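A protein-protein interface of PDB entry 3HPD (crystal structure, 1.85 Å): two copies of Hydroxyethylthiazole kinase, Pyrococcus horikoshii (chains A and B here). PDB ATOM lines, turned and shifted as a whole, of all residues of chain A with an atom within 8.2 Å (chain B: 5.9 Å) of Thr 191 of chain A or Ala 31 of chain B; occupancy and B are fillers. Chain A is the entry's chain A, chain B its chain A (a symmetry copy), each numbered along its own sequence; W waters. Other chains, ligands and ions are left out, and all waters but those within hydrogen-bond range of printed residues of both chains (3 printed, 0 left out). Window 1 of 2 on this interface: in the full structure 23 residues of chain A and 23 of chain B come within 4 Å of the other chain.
Val 25 of chain A touches Met 27 of chain B.
CG of Met 43 of chain B touches CG2 of Val 25 of chain A, 3.9 Å away.
ND2 of Asn 28 of chain B touches OG1 of Thr 29 of chain A (3.7 Å).
Gly 188 of chain A touches Leu 35 of chain B (O to CD2, 3.8 Å).
CA of Val 190 of chain A touches OD1 of Asn 32 of chain B (3.5 Å).
C of Val 190 of chain A touches CD1 of Leu 35 of chain B, 3.5 Å away.
Thr 191 of chain A touches Asn 28 of chain B.
Thr 191 of chain A touches Ala 31 of chain B.
Thr 191 of chain A touches Leu 35 of chain B (N to CD1, 3.2 Å).
ND1 of His 239 of chain A touches ND2 of Asn 32 of chain B, at 3.9 Å.
Positions printed for both chains: 26, 29 and 30.
The backbone NH of Val 25 of chain A is in hydrogen-bond range of the side-chain amide oxygen of Asn 23 of chain A (2.8 Å).
NE2 of His 239 of chain A is in hydrogen-bond range of OG1 of Thr 29 of chain A (3.5 Å).
OG1 of Thr 29 of chain A is in hydrogen-bond range of OH of Tyr 243 of chain A (2.9 Å).
The side-chain hydroxyl (OH) of Tyr 243 of chain A lies within hydrogen-bond range of a ring nitrogen (NE2) of His 239 of chain A, at 2.7 Å.
The side-chain amide oxygen (OD1) of Asn 28 of chain B lies within hydrogen-bond range of the side-chain amide nitrogen (ND2) of Asn 32 of chain B (2.9 Å).
Water W2 lies within hydrogen-bond range of the backbone carbonyl oxygen of Arg 189 of chain A (2.7 Å) and the backbone carbonyl oxygen of Asn 32 of chain B (2.8 Å).
Water W1 lies within hydrogen-bond range of O of Thr 191 of chain A, ND2 of Asn 32 of chain B, ND2 of Asn 28 of chain B and NE2 of His 239 of chain A.
Water W3 bridges the guanidinium group (NH1) of Arg 189 of chain A (3.0 Å) and the backbone carbonyl oxygen (O) of Ala 36 of chain B (3.2 Å).
The backbone carbonyl oxygen (O) of Val 25 of chain A lies within hydrogen-bond range of the side-chain amide nitrogen (ND2) of Asn 28 of chain B.
The backbone carbonyl oxygen (O) of Leu 35 of chain B lies within hydrogen-bond range of the guanidinium group (NH1) of Arg 189 of chain A (3.0 Å).
The guanidinium group (NH1) of Arg 189 of chain A sits at hydrogen-bond distance from the backbone carbonyl oxygen (O) of Ala 36 of chain B (3.5 Å).
OD1 of Asn 32 of chain B sits at hydrogen-bond distance from N of Thr 191 of chain A, at 2.7 Å.
Of the 13 printed residues of chain B, 7 touch a printed residue of chain A.
Hydrophobic or aromatic side chains of chain B that line the printed part of chain A: Met 27, Ala 31, Leu 35 and Met 43.
Along chain B the printed residues that touch a printed residue of chain A span positions 27 to 43.
Of the 21 printed residues of chain A, 7 touch a printed residue of chain B.
Printed residues of chain A that touch a printed residue of chain B: Val 25, Thr 29, Gly 188, Arg 189, Val 190, Thr 191 and His 239.
Hydrophobic or aromatic side chains of chain A within 4 Å of the printed part of chain B: Val 25 and His 239.
Along chain A the printed residues that touch a printed residue of chain B span positions 25 to 239.
Among the printed residues, 14 pairs touch across the chains.
Among the printed residues, no Asp or Glu carboxylate lies within 4 Å of a Lys or Arg side-chain nitrogen of the other chain.
Ala 31 of chain B touches just one residue of chain A: Thr 191.
Of chain A, only Val 190 (3.5 Å), Thr 191 (2.7 Å) and His 239 (3.9 Å) come within 4 Å of Asn 32 of chain B.
Printed residues of chain A within 4 Å of Ala 36 of chain B: Arg 189.
Of the printed residues of chain B, Arg 189 of chain A touches Leu 35 and Ala 36.
Of the printed residues of chain A, Met 27 of chain B touches Val 25.
Of the printed residues of chain A, Asn 28 of chain B touches Val 25 (2.9 Å), Thr 29 (3.7 Å) and Thr 191 (3.5 Å).
Printed residues of chain A within 4 Å of Leu 35 of chain B: Gly 188 (3.8 Å), Arg 189 (3.0 Å), Val 190 (3.5 Å) and Thr 191 (3.2 Å).
The nearest residue of chain A that does not touch Ala 31 of chain B is Val 25 of chain A (4.2 Å).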
ATOM      1  N   ASN A  23       7.896  34.281  -6.076  1.00  0.00           N
ATOM      2  CA  ASN A  23       6.468  34.513  -6.285  1.00  0.00           C
ATOM      3  C   ASN A  23       5.559  33.575  -5.492  1.00  0.00           C
ATOM      4  O   ASN A  23       5.951  32.473  -5.114  1.00  0.00           O
ATOM      5  CB  ASN A  23       6.134  34.490  -7.792  1.00  0.00           C
ATOM      6  CG  ASN A  23       6.047  33.088  -8.372  1.00  0.00           C
ATOM      7  OD1 ASN A  23       5.171  32.310  -8.007  1.00  0.00           O
ATOM      8  ND2 ASN A  23       6.949  32.772  -9.301  1.00  0.00           N
ATOM      9  N   VAL A  25       3.051  31.705  -6.239  1.00  0.00           N
ATOM     10  CA  VAL A  25       2.671  30.423  -6.814  1.00  0.00           C
ATOM     11  C   VAL A  25       3.715  29.334  -6.585  1.00  0.00           C
ATOM     12  O   VAL A  25       3.376  28.152  -6.513  1.00  0.00           O
ATOM     13  CB  VAL A  25       2.431  30.563  -8.342  1.00  0.00           C
ATOM     14  CG1 VAL A  25       2.012  29.225  -8.942  1.00  0.00           C
ATOM     15  CG2 VAL A  25       1.373  31.616  -8.604  1.00  0.00           C
ATOM     16  N   VAL A  26       4.976  29.730  -6.441  1.00  0.00           N
ATOM     17  CA  VAL A  26       6.047  28.745  -6.287  1.00  0.00           C
ATOM     18  C   VAL A  26       6.758  28.692  -4.936  1.00  0.00           C
ATOM     19  O   VAL A  26       7.793  28.037  -4.804  1.00  0.00           O
ATOM     20  CB  VAL A  26       7.106  28.944  -7.392  1.00  0.00           C
ATOM     21  CG1 VAL A  26       6.416  29.022  -8.754  1.00  0.00           C
ATOM     22  CG2 VAL A  26       7.913  30.217  -7.128  1.00  0.00           C
ATOM     23  N   THR A  29       6.607  24.985  -3.571  1.00  0.00           N
ATOM     24  CA  THR A  29       7.117  24.205  -4.659  1.00  0.00           C
ATOM     25  C   THR A  29       8.651  24.324  -4.847  1.00  0.00           C
ATOM     26  O   THR A  29       9.358  23.306  -4.908  1.00  0.00           O
ATOM     27  CB  THR A  29       6.260  24.628  -5.874  1.00  0.00           C
ATOM     28  OG1 THR A  29       5.460  23.524  -6.309  1.00  0.00           O
ATOM     29  CG2 THR A  29       7.072  25.207  -6.931  1.00  0.00           C
ATOM     30  N   THR A  30       9.187  25.542  -4.889  1.00  0.00           N
ATOM     31  CA  THR A  30      10.635  25.701  -5.053  1.00  0.00           C
ATOM     32  C   THR A  30      11.396  25.356  -3.772  1.00  0.00           C
ATOM     33  O   THR A  30      12.551  24.919  -3.825  1.00  0.00           O
ATOM     34  CB  THR A  30      11.010  27.139  -5.499  1.00  0.00           C
ATOM     35  OG1 THR A  30      10.534  28.091  -4.540  1.00  0.00           O
ATOM     36  CG2 THR A  30      10.400  27.445  -6.861  1.00  0.00           C
ATOM     37  N   LEU A 186       5.696  17.075 -20.485  1.00  0.00           N
ATOM     38  CA  LEU A 186       4.650  17.178 -19.469  1.00  0.00           C
ATOM     39  C   LEU A 186       4.947  18.296 -18.468  1.00  0.00           C
ATOM     40  O   LEU A 186       4.064  18.716 -17.721  1.00  0.00           O
ATOM     41  CB  LEU A 186       4.457  15.842 -18.736  1.00  0.00           C
ATOM     42  CG  LEU A 186       3.181  15.751 -17.886  1.00  0.00           C
ATOM     43  CD1 LEU A 186       1.960  16.023 -18.762  1.00  0.00           C
ATOM     44  CD2 LEU A 186       3.076  14.378 -17.250  1.00  0.00           C
ATOM     45  N   LEU A 187       6.187  18.777 -18.456  1.00  0.00           N
ATOM     46  CA  LEU A 187       6.555  19.868 -17.562  1.00  0.00           C
ATOM     47  C   LEU A 187       5.667  21.061 -17.889  1.00  0.00           C
ATOM     48  O   LEU A 187       5.442  21.929 -17.048  1.00  0.00           O
ATOM     49  CB  LEU A 187       8.027  20.263 -17.746  1.00  0.00           C
ATOM     50  CG  LEU A 187       9.089  19.365 -17.103  1.00  0.00           C
ATOM     51  CD1 LEU A 187      10.476  19.876 -17.469  1.00  0.00           C
ATOM     52  CD2 LEU A 187       8.917  19.351 -15.583  1.00  0.00           C
ATOM     53  N   GLY A 188       5.165  21.095 -19.121  1.00  0.00           N
ATOM     54  CA  GLY A 188       4.302  22.185 -19.532  1.00  0.00           C
ATOM     55  C   GLY A 188       2.965  22.190 -18.810  1.00  0.00           C
ATOM     56  O   GLY A 188       2.229  23.179 -18.868  1.00  0.00           O
ATOM     57  N   ARG A 189       2.644  21.093 -18.128  1.00  0.00           N
ATOM     58  CA  ARG A 189       1.380  20.994 -17.402  1.00  0.00           C
ATOM     59  C   ARG A 189       1.542  21.145 -15.894  1.00  0.00           C
ATOM     60  O   ARG A 189       0.612  20.885 -15.129  1.00  0.00           O
ATOM     61  CB  ARG A 189       0.684  19.665 -17.715  1.00  0.00           C
ATOM     62  CG  ARG A 189       0.343  19.472 -19.183  1.00  0.00           C
ATOM     63  CD  ARG A 189      -0.393  20.675 -19.765  1.00  0.00           C
ATOM     64  NE  ARG A 189      -0.907  20.384 -21.099  1.00  0.00           N
ATOM     65  CZ  ARG A 189      -2.143  19.967 -21.353  1.00  0.00           C
ATOM     66  NH1 ARG A 189      -3.009  19.804 -20.362  1.00  0.00           N
ATOM     67  NH2 ARG A 189      -2.506  19.693 -22.599  1.00  0.00           N
ATOM     68  N   VAL A 190       2.731  21.559 -15.468  1.00  0.00           N
ATOM     69  CA  VAL A 190       3.001  21.781 -14.052  1.00  0.00           C
ATOM     70  C   VAL A 190       3.493  23.223 -13.966  1.00  0.00           C
ATOM     71  O   VAL A 190       4.428  23.606 -14.662  1.00  0.00           O
ATOM     72  CB  VAL A 190       4.081  20.819 -13.522  1.00  0.00           C
ATOM     73  CG1 VAL A 190       4.311  21.055 -12.029  1.00  0.00           C
ATOM     74  CG2 VAL A 190       3.644  19.376 -13.758  1.00  0.00           C
ATOM     75  N   THR A 191       2.867  24.028 -13.119  1.00  0.00           N
ATOM     76  CA  THR A 191       3.252  25.427 -13.025  1.00  0.00           C
ATOM     77  C   THR A 191       4.562  25.694 -12.288  1.00  0.00           C
ATOM     78  O   THR A 191       4.907  25.009 -11.320  1.00  0.00           O
ATOM     79  CB  THR A 191       2.126  26.266 -12.373  1.00  0.00           C
ATOM     80  OG1 THR A 191       2.376  27.659 -12.611  1.00  0.00           O
ATOM     81  CG2 THR A 191       2.062  26.012 -10.870  1.00  0.00           C
ATOM     82  N   GLY A 192       5.292  26.698 -12.770  1.00  0.00           N
ATOM     83  CA  GLY A 192       6.546  27.087 -12.150  1.00  0.00           C
ATOM     84  C   GLY A 192       7.706  26.113 -12.233  1.00  0.00           C
ATOM     85  O   GLY A 192       8.552  26.086 -11.336  1.00  0.00           O
ATOM     86  N   THR A 193       7.767  25.309 -13.291  1.00  0.00           N
ATOM     87  CA  THR A 193       8.871  24.367 -13.423  1.00  0.00           C
ATOM     88  C   THR A 193      10.161  25.109 -13.768  1.00  0.00           C
ATOM     89  O   THR A 193      11.243  24.739 -13.312  1.00  0.00           O
ATOM     90  CB  THR A 193       8.570  23.286 -14.478  1.00  0.00           C
ATOM     91  OG1 THR A 193       8.083  23.899 -15.675  1.00  0.00           O
ATOM     92  CG2 THR A 193       7.525  22.306 -13.942  1.00  0.00           C
ATOM     93  N   GLY A 194      10.050  26.165 -14.567  1.00  0.00           N
ATOM     94  CA  GLY A 194      11.231  26.941 -14.898  1.00  0.00           C
ATOM     95  C   GLY A 194      11.716  27.619 -13.627  1.00  0.00           C
ATOM     96  O   GLY A 194      12.917  27.819 -13.425  1.00  0.00           O
ATOM     97  N   CYS A 195      10.770  27.966 -12.758  1.00  0.00           N
ATOM     98  CA  CYS A 195      11.094  28.618 -11.496  1.00  0.00           C
ATOM     99  C   CYS A 195      11.808  27.626 -10.582  1.00  0.00           C
ATOM    100  O   CYS A 195      12.657  28.012  -9.778  1.00  0.00           O
ATOM    101  CB  CYS A 195       9.821  29.148 -10.830  1.00  0.00           C
ATOM    102  SG  CYS A 195       8.944  30.397 -11.831  1.00  0.00           S
ATOM    103  N   MET A 196      11.458  26.349 -10.703  1.00  0.00           N
ATOM    104  CA  MET A 196      12.116  25.320  -9.906  1.00  0.00           C
ATOM    105  C   MET A 196      13.574  25.270 -10.344  1.00  0.00           C
ATOM    106  O   MET A 196      14.479  25.162  -9.520  1.00  0.00           O
ATOM    107  CB  MET A 196      11.478  23.949 -10.141  1.00  0.00           C
ATOM    108  CG  MET A 196      10.076  23.793  -9.579  1.00  0.00           C
ATOM    109  SD  MET A 196       9.424  22.149  -9.966  1.00  0.00           S
ATOM    110  CE  MET A 196       8.028  22.072  -8.860  1.00  0.00           C
ATOM    111  N   PHE A 221      17.528  18.641 -13.433  1.00  0.00           N
ATOM    112  CA  PHE A 221      16.073  18.771 -13.432  1.00  0.00           C
ATOM    113  C   PHE A 221      15.451  18.085 -14.643  1.00  0.00           C
ATOM    114  O   PHE A 221      14.378  17.485 -14.549  1.00  0.00           O
ATOM    115  CB  PHE A 221      15.666  20.246 -13.420  1.00  0.00           C
ATOM    116  CG  PHE A 221      14.190  20.461 -13.242  1.00  0.00           C
ATOM    117  CD1 PHE A 221      13.595  20.274 -11.999  1.00  0.00           C
ATOM    118  CD2 PHE A 221      13.391  20.820 -14.323  1.00  0.00           C
ATOM    119  CE1 PHE A 221      12.221  20.447 -11.829  1.00  0.00           C
ATOM    120  CE2 PHE A 221      12.013  20.996 -14.165  1.00  0.00           C
ATOM    121  CZ  PHE A 221      11.429  20.807 -12.917  1.00  0.00           C
ATOM    122  N   PRO A 235      -0.250  14.938 -14.925  1.00  0.00           N
ATOM    123  CA  PRO A 235       0.167  16.143 -14.192  1.00  0.00           C
ATOM    124  C   PRO A 235       0.302  16.120 -12.672  1.00  0.00           C
ATOM    125  O   PRO A 235       1.310  16.587 -12.139  1.00  0.00           O
ATOM    126  CB  PRO A 235      -0.835  17.199 -14.659  1.00  0.00           C
ATOM    127  CG  PRO A 235      -1.169  16.762 -16.035  1.00  0.00           C
ATOM    128  CD  PRO A 235      -1.341  15.270 -15.858  1.00  0.00           C
ATOM    129  N   HIS A 239       3.980  15.679 -11.017  1.00  0.00           N
ATOM    130  CA  HIS A 239       4.514  16.763 -10.191  1.00  0.00           C
ATOM    131  C   HIS A 239       5.166  16.193  -8.929  1.00  0.00           C
ATOM    132  O   HIS A 239       6.275  16.582  -8.560  1.00  0.00           O
ATOM    133  CB  HIS A 239       3.382  17.726  -9.797  1.00  0.00           C
ATOM    134  CG  HIS A 239       3.833  18.899  -8.981  1.00  0.00           C
ATOM    135  ND1 HIS A 239       2.948  19.745  -8.345  1.00  0.00           N
ATOM    136  CD2 HIS A 239       5.071  19.374  -8.700  1.00  0.00           C
ATOM    137  CE1 HIS A 239       3.621  20.686  -7.708  1.00  0.00           C
ATOM    138  NE2 HIS A 239       4.912  20.484  -7.908  1.00  0.00           N
ATOM    139  N   LEU A 242       8.585  14.568  -9.360  1.00  0.00           N
ATOM    140  CA  LEU A 242       9.715  15.447  -9.645  1.00  0.00           C
ATOM    141  C   LEU A 242      10.596  15.565  -8.399  1.00  0.00           C
ATOM    142  O   LEU A 242      11.822  15.490  -8.481  1.00  0.00           O
ATOM    143  CB  LEU A 242       9.233  16.839 -10.079  1.00  0.00           C
ATOM    144  CG  LEU A 242       8.531  16.924 -11.444  1.00  0.00           C
ATOM    145  CD1 LEU A 242       8.056  18.355 -11.694  1.00  0.00           C
ATOM    146  CD2 LEU A 242       9.493  16.479 -12.544  1.00  0.00           C
ATOM    147  N   TYR A 243       9.962  15.741  -7.242  1.00  0.00           N
ATOM    148  CA  TYR A 243      10.691  15.858  -5.981  1.00  0.00           C
ATOM    149  C   TYR A 243      11.370  14.541  -5.645  1.00  0.00           C
ATOM    150  O   TYR A 243      12.494  14.526  -5.144  1.00  0.00           O
ATOM    151  CB  TYR A 243       9.732  16.231  -4.852  1.00  0.00           C
ATOM    152  CG  TYR A 243       8.954  17.485  -5.144  1.00  0.00           C
ATOM    153  CD1 TYR A 243       9.562  18.740  -5.065  1.00  0.00           C
ATOM    154  CD2 TYR A 243       7.621  17.420  -5.547  1.00  0.00           C
ATOM    155  CE1 TYR A 243       8.862  19.901  -5.383  1.00  0.00           C
ATOM    156  CE2 TYR A 243       6.908  18.580  -5.869  1.00  0.00           C
ATOM    157  CZ  TYR A 243       7.536  19.814  -5.783  1.00  0.00           C
ATOM    158  OH  TYR A 243       6.836  20.965  -6.080  1.00  0.00           O
ATOM    159  N   VAL B  26      -4.464  29.143  -2.468  1.00  0.00           N
ATOM    160  CA  VAL B  26      -4.735  28.436  -3.720  1.00  0.00           C
ATOM    161  C   VAL B  26      -3.927  28.852  -4.947  1.00  0.00           C
ATOM    162  O   VAL B  26      -4.244  28.446  -6.067  1.00  0.00           O
ATOM    163  CB  VAL B  26      -6.236  28.533  -4.063  1.00  0.00           C
ATOM    164  CG1 VAL B  26      -7.068  28.141  -2.842  1.00  0.00           C
ATOM    165  CG2 VAL B  26      -6.585  29.953  -4.513  1.00  0.00           C
ATOM    166  N   MET B  27      -2.881  29.643  -4.738  1.00  0.00           N
ATOM    167  CA  MET B  27      -2.034  30.109  -5.835  1.00  0.00           C
ATOM    168  C   MET B  27      -1.524  28.993  -6.749  1.00  0.00           C
ATOM    169  O   MET B  27      -1.753  29.012  -7.956  1.00  0.00           O
ATOM    170  CB  MET B  27      -0.830  30.874  -5.273  1.00  0.00           C
ATOM    171  CG  MET B  27      -1.132  32.279  -4.757  1.00  0.00           C
ATOM    172  SD  MET B  27      -1.201  33.523  -6.071  1.00  0.00           S
ATOM    173  CE  MET B  27      -1.842  34.950  -5.149  1.00  0.00           C
ATOM    174  N   ASN B  28      -0.831  28.023  -6.164  1.00  0.00           N
ATOM    175  CA  ASN B  28      -0.255  26.913  -6.923  1.00  0.00           C
ATOM    176  C   ASN B  28      -1.303  25.926  -7.395  1.00  0.00           C
ATOM    177  O   ASN B  28      -1.310  25.435  -8.523  1.00  0.00           O
ATOM    178  CB  ASN B  28       0.743  26.177  -6.037  1.00  0.00           C
ATOM    179  CG  ASN B  28       1.487  25.100  -6.778  1.00  0.00           C
ATOM    180  OD1 ASN B  28       1.096  23.933  -6.775  1.00  0.00           O
ATOM    181  ND2 ASN B  28       2.558  25.493  -7.446  1.00  0.00           N
ATOM    182  N   THR B  29      -2.186  25.644  -6.466  1.00  0.00           N
ATOM    183  CA  THR B  29      -3.267  24.718  -6.623  1.00  0.00           C
ATOM    184  C   THR B  29      -4.211  25.055  -7.806  1.00  0.00           C
ATOM    185  O   THR B  29      -4.480  24.196  -8.661  1.00  0.00           O
ATOM    186  CB  THR B  29      -3.936  24.661  -5.230  1.00  0.00           C
ATOM    187  OG1 THR B  29      -3.761  23.359  -4.662  1.00  0.00           O
ATOM    188  CG2 THR B  29      -5.323  25.089  -5.280  1.00  0.00           C
ATOM    189  N   THR B  30      -4.678  26.297  -7.903  1.00  0.00           N
ATOM    190  CA  THR B  30      -5.563  26.664  -9.012  1.00  0.00           C
ATOM    191  C   THR B  30      -4.802  26.794 -10.332  1.00  0.00           C
ATOM    192  O   THR B  30      -5.365  26.570 -11.409  1.00  0.00           O
ATOM    193  CB  THR B  30      -6.326  27.986  -8.729  1.00  0.00           C
ATOM    194  OG1 THR B  30      -5.395  29.049  -8.495  1.00  0.00           O
ATOM    195  CG2 THR B  30      -7.227  27.825  -7.513  1.00  0.00           C
ATOM    196  N   ALA B  31      -3.522  27.151 -10.250  1.00  0.00           N
ATOM    197  CA  ALA B  31      -2.698  27.277 -11.446  1.00  0.00           C
ATOM    198  C   ALA B  31      -2.528  25.896 -12.067  1.00  0.00           C
ATOM    199  O   ALA B  31      -2.667  25.728 -13.278  1.00  0.00           O
ATOM    200  CB  ALA B  31      -1.335  27.856 -11.098  1.00  0.00           C
ATOM    201  N   ASN B  32      -2.229  24.905 -11.230  1.00  0.00           N
ATOM    202  CA  ASN B  32      -2.053  23.551 -11.723  1.00  0.00           C
ATOM    203  C   ASN B  32      -3.361  22.921 -12.178  1.00  0.00           C
ATOM    204  O   ASN B  32      -3.363  22.061 -13.057  1.00  0.00           O
ATOM    205  CB  ASN B  32      -1.373  22.676 -10.671  1.00  0.00           C
ATOM    206  CG  ASN B  32       0.128  22.866 -10.653  1.00  0.00           C
ATOM    207  OD1 ASN B  32       0.744  23.060 -11.703  1.00  0.00           O
ATOM    208  ND2 ASN B  32       0.726  22.797  -9.470  1.00  0.00           N
ATOM    209  N   ALA B  33      -4.473  23.341 -11.584  1.00  0.00           N
ATOM    210  CA  ALA B  33      -5.768  22.811 -11.993  1.00  0.00           C
ATOM    211  C   ALA B  33      -6.034  23.307 -13.415  1.00  0.00           C
ATOM    212  O   ALA B  33      -6.484  22.548 -14.277  1.00  0.00           O
ATOM    213  CB  ALA B  33      -6.865  23.287 -11.042  1.00  0.00           C
ATOM    214  N   LEU B  34      -5.748  24.583 -13.662  1.00  0.00           N
ATOM    215  CA  LEU B  34      -5.949  25.155 -14.988  1.00  0.00           C
ATOM    216  C   LEU B  34      -5.043  24.490 -16.022  1.00  0.00           C
ATOM    217  O   LEU B  34      -5.485  24.175 -17.124  1.00  0.00           O
ATOM    218  CB  LEU B  34      -5.700  26.668 -14.963  1.00  0.00           C
ATOM    219  CG  LEU B  34      -6.891  27.502 -14.480  1.00  0.00           C
ATOM    220  CD1 LEU B  34      -6.444  28.906 -14.098  1.00  0.00           C
ATOM    221  CD2 LEU B  34      -7.943  27.546 -15.581  1.00  0.00           C
ATOM    222  N   LEU B  35      -3.778  24.273 -15.673  1.00  0.00           N
ATOM    223  CA  LEU B  35      -2.853  23.632 -16.611  1.00  0.00           C
ATOM    224  C   LEU B  35      -3.288  22.200 -16.939  1.00  0.00           C
ATOM    225  O   LEU B  35      -3.215  21.771 -18.088  1.00  0.00           O
ATOM    226  CB  LEU B  35      -1.428  23.618 -16.045  1.00  0.00           C
ATOM    227  CG  LEU B  35      -0.680  24.956 -16.024  1.00  0.00           C
ATOM    228  CD1 LEU B  35       0.635  24.777 -15.275  1.00  0.00           C
ATOM    229  CD2 LEU B  35      -0.425  25.448 -17.445  1.00  0.00           C
ATOM    230  N   ALA B  36      -3.743  21.464 -15.931  1.00  0.00           N
ATOM    231  CA  ALA B  36      -4.181  20.088 -16.149  1.00  0.00           C
ATOM    232  C   ALA B  36      -5.380  20.043 -17.093  1.00  0.00           C
ATOM    233  O   ALA B  36      -5.465  19.168 -17.957  1.00  0.00           O
ATOM    234  CB  ALA B  36      -4.540  19.429 -14.814  1.00  0.00           C
ATOM    235  N   PRO B  41      -2.642  29.532 -16.832  1.00  0.00           N
ATOM    236  CA  PRO B  41      -2.899  30.498 -15.766  1.00  0.00           C
ATOM    237  C   PRO B  41      -1.847  31.595 -15.703  1.00  0.00           C
ATOM    238  O   PRO B  41      -0.726  31.433 -16.182  1.00  0.00           O
ATOM    239  CB  PRO B  41      -2.834  29.635 -14.520  1.00  0.00           C
ATOM    240  CG  PRO B  41      -1.651  28.747 -14.847  1.00  0.00           C
ATOM    241  CD  PRO B  41      -1.923  28.355 -16.302  1.00  0.00           C
ATOM    242  N   MET B  43      -0.999  34.559 -12.601  1.00  0.00           N
ATOM    243  CA  MET B  43      -1.362  35.210 -11.351  1.00  0.00           C
ATOM    244  C   MET B  43      -0.640  36.552 -11.286  1.00  0.00           C
ATOM    245  O   MET B  43       0.589  36.606 -11.328  1.00  0.00           O
ATOM    246  CB  MET B  43      -0.958  34.341 -10.154  1.00  0.00           C
ATOM    247  CG  MET B  43      -1.967  33.253  -9.783  1.00  0.00           C
ATOM    248  SD  MET B  43      -2.300  32.080 -11.107  1.00  0.00           S
ATOM    249  CE  MET B  43      -3.476  30.988 -10.300  1.00  0.00           C
HETATM  250  O   HOH W   1       3.753  23.409  -9.397  1.00  0.00           O
HETATM  251  O   HOH W   2      -1.291  20.251 -13.343  1.00  0.00           O
HETATM  252  O   HOH W   3      -5.763  18.739 -21.077  1.00  0.00           O
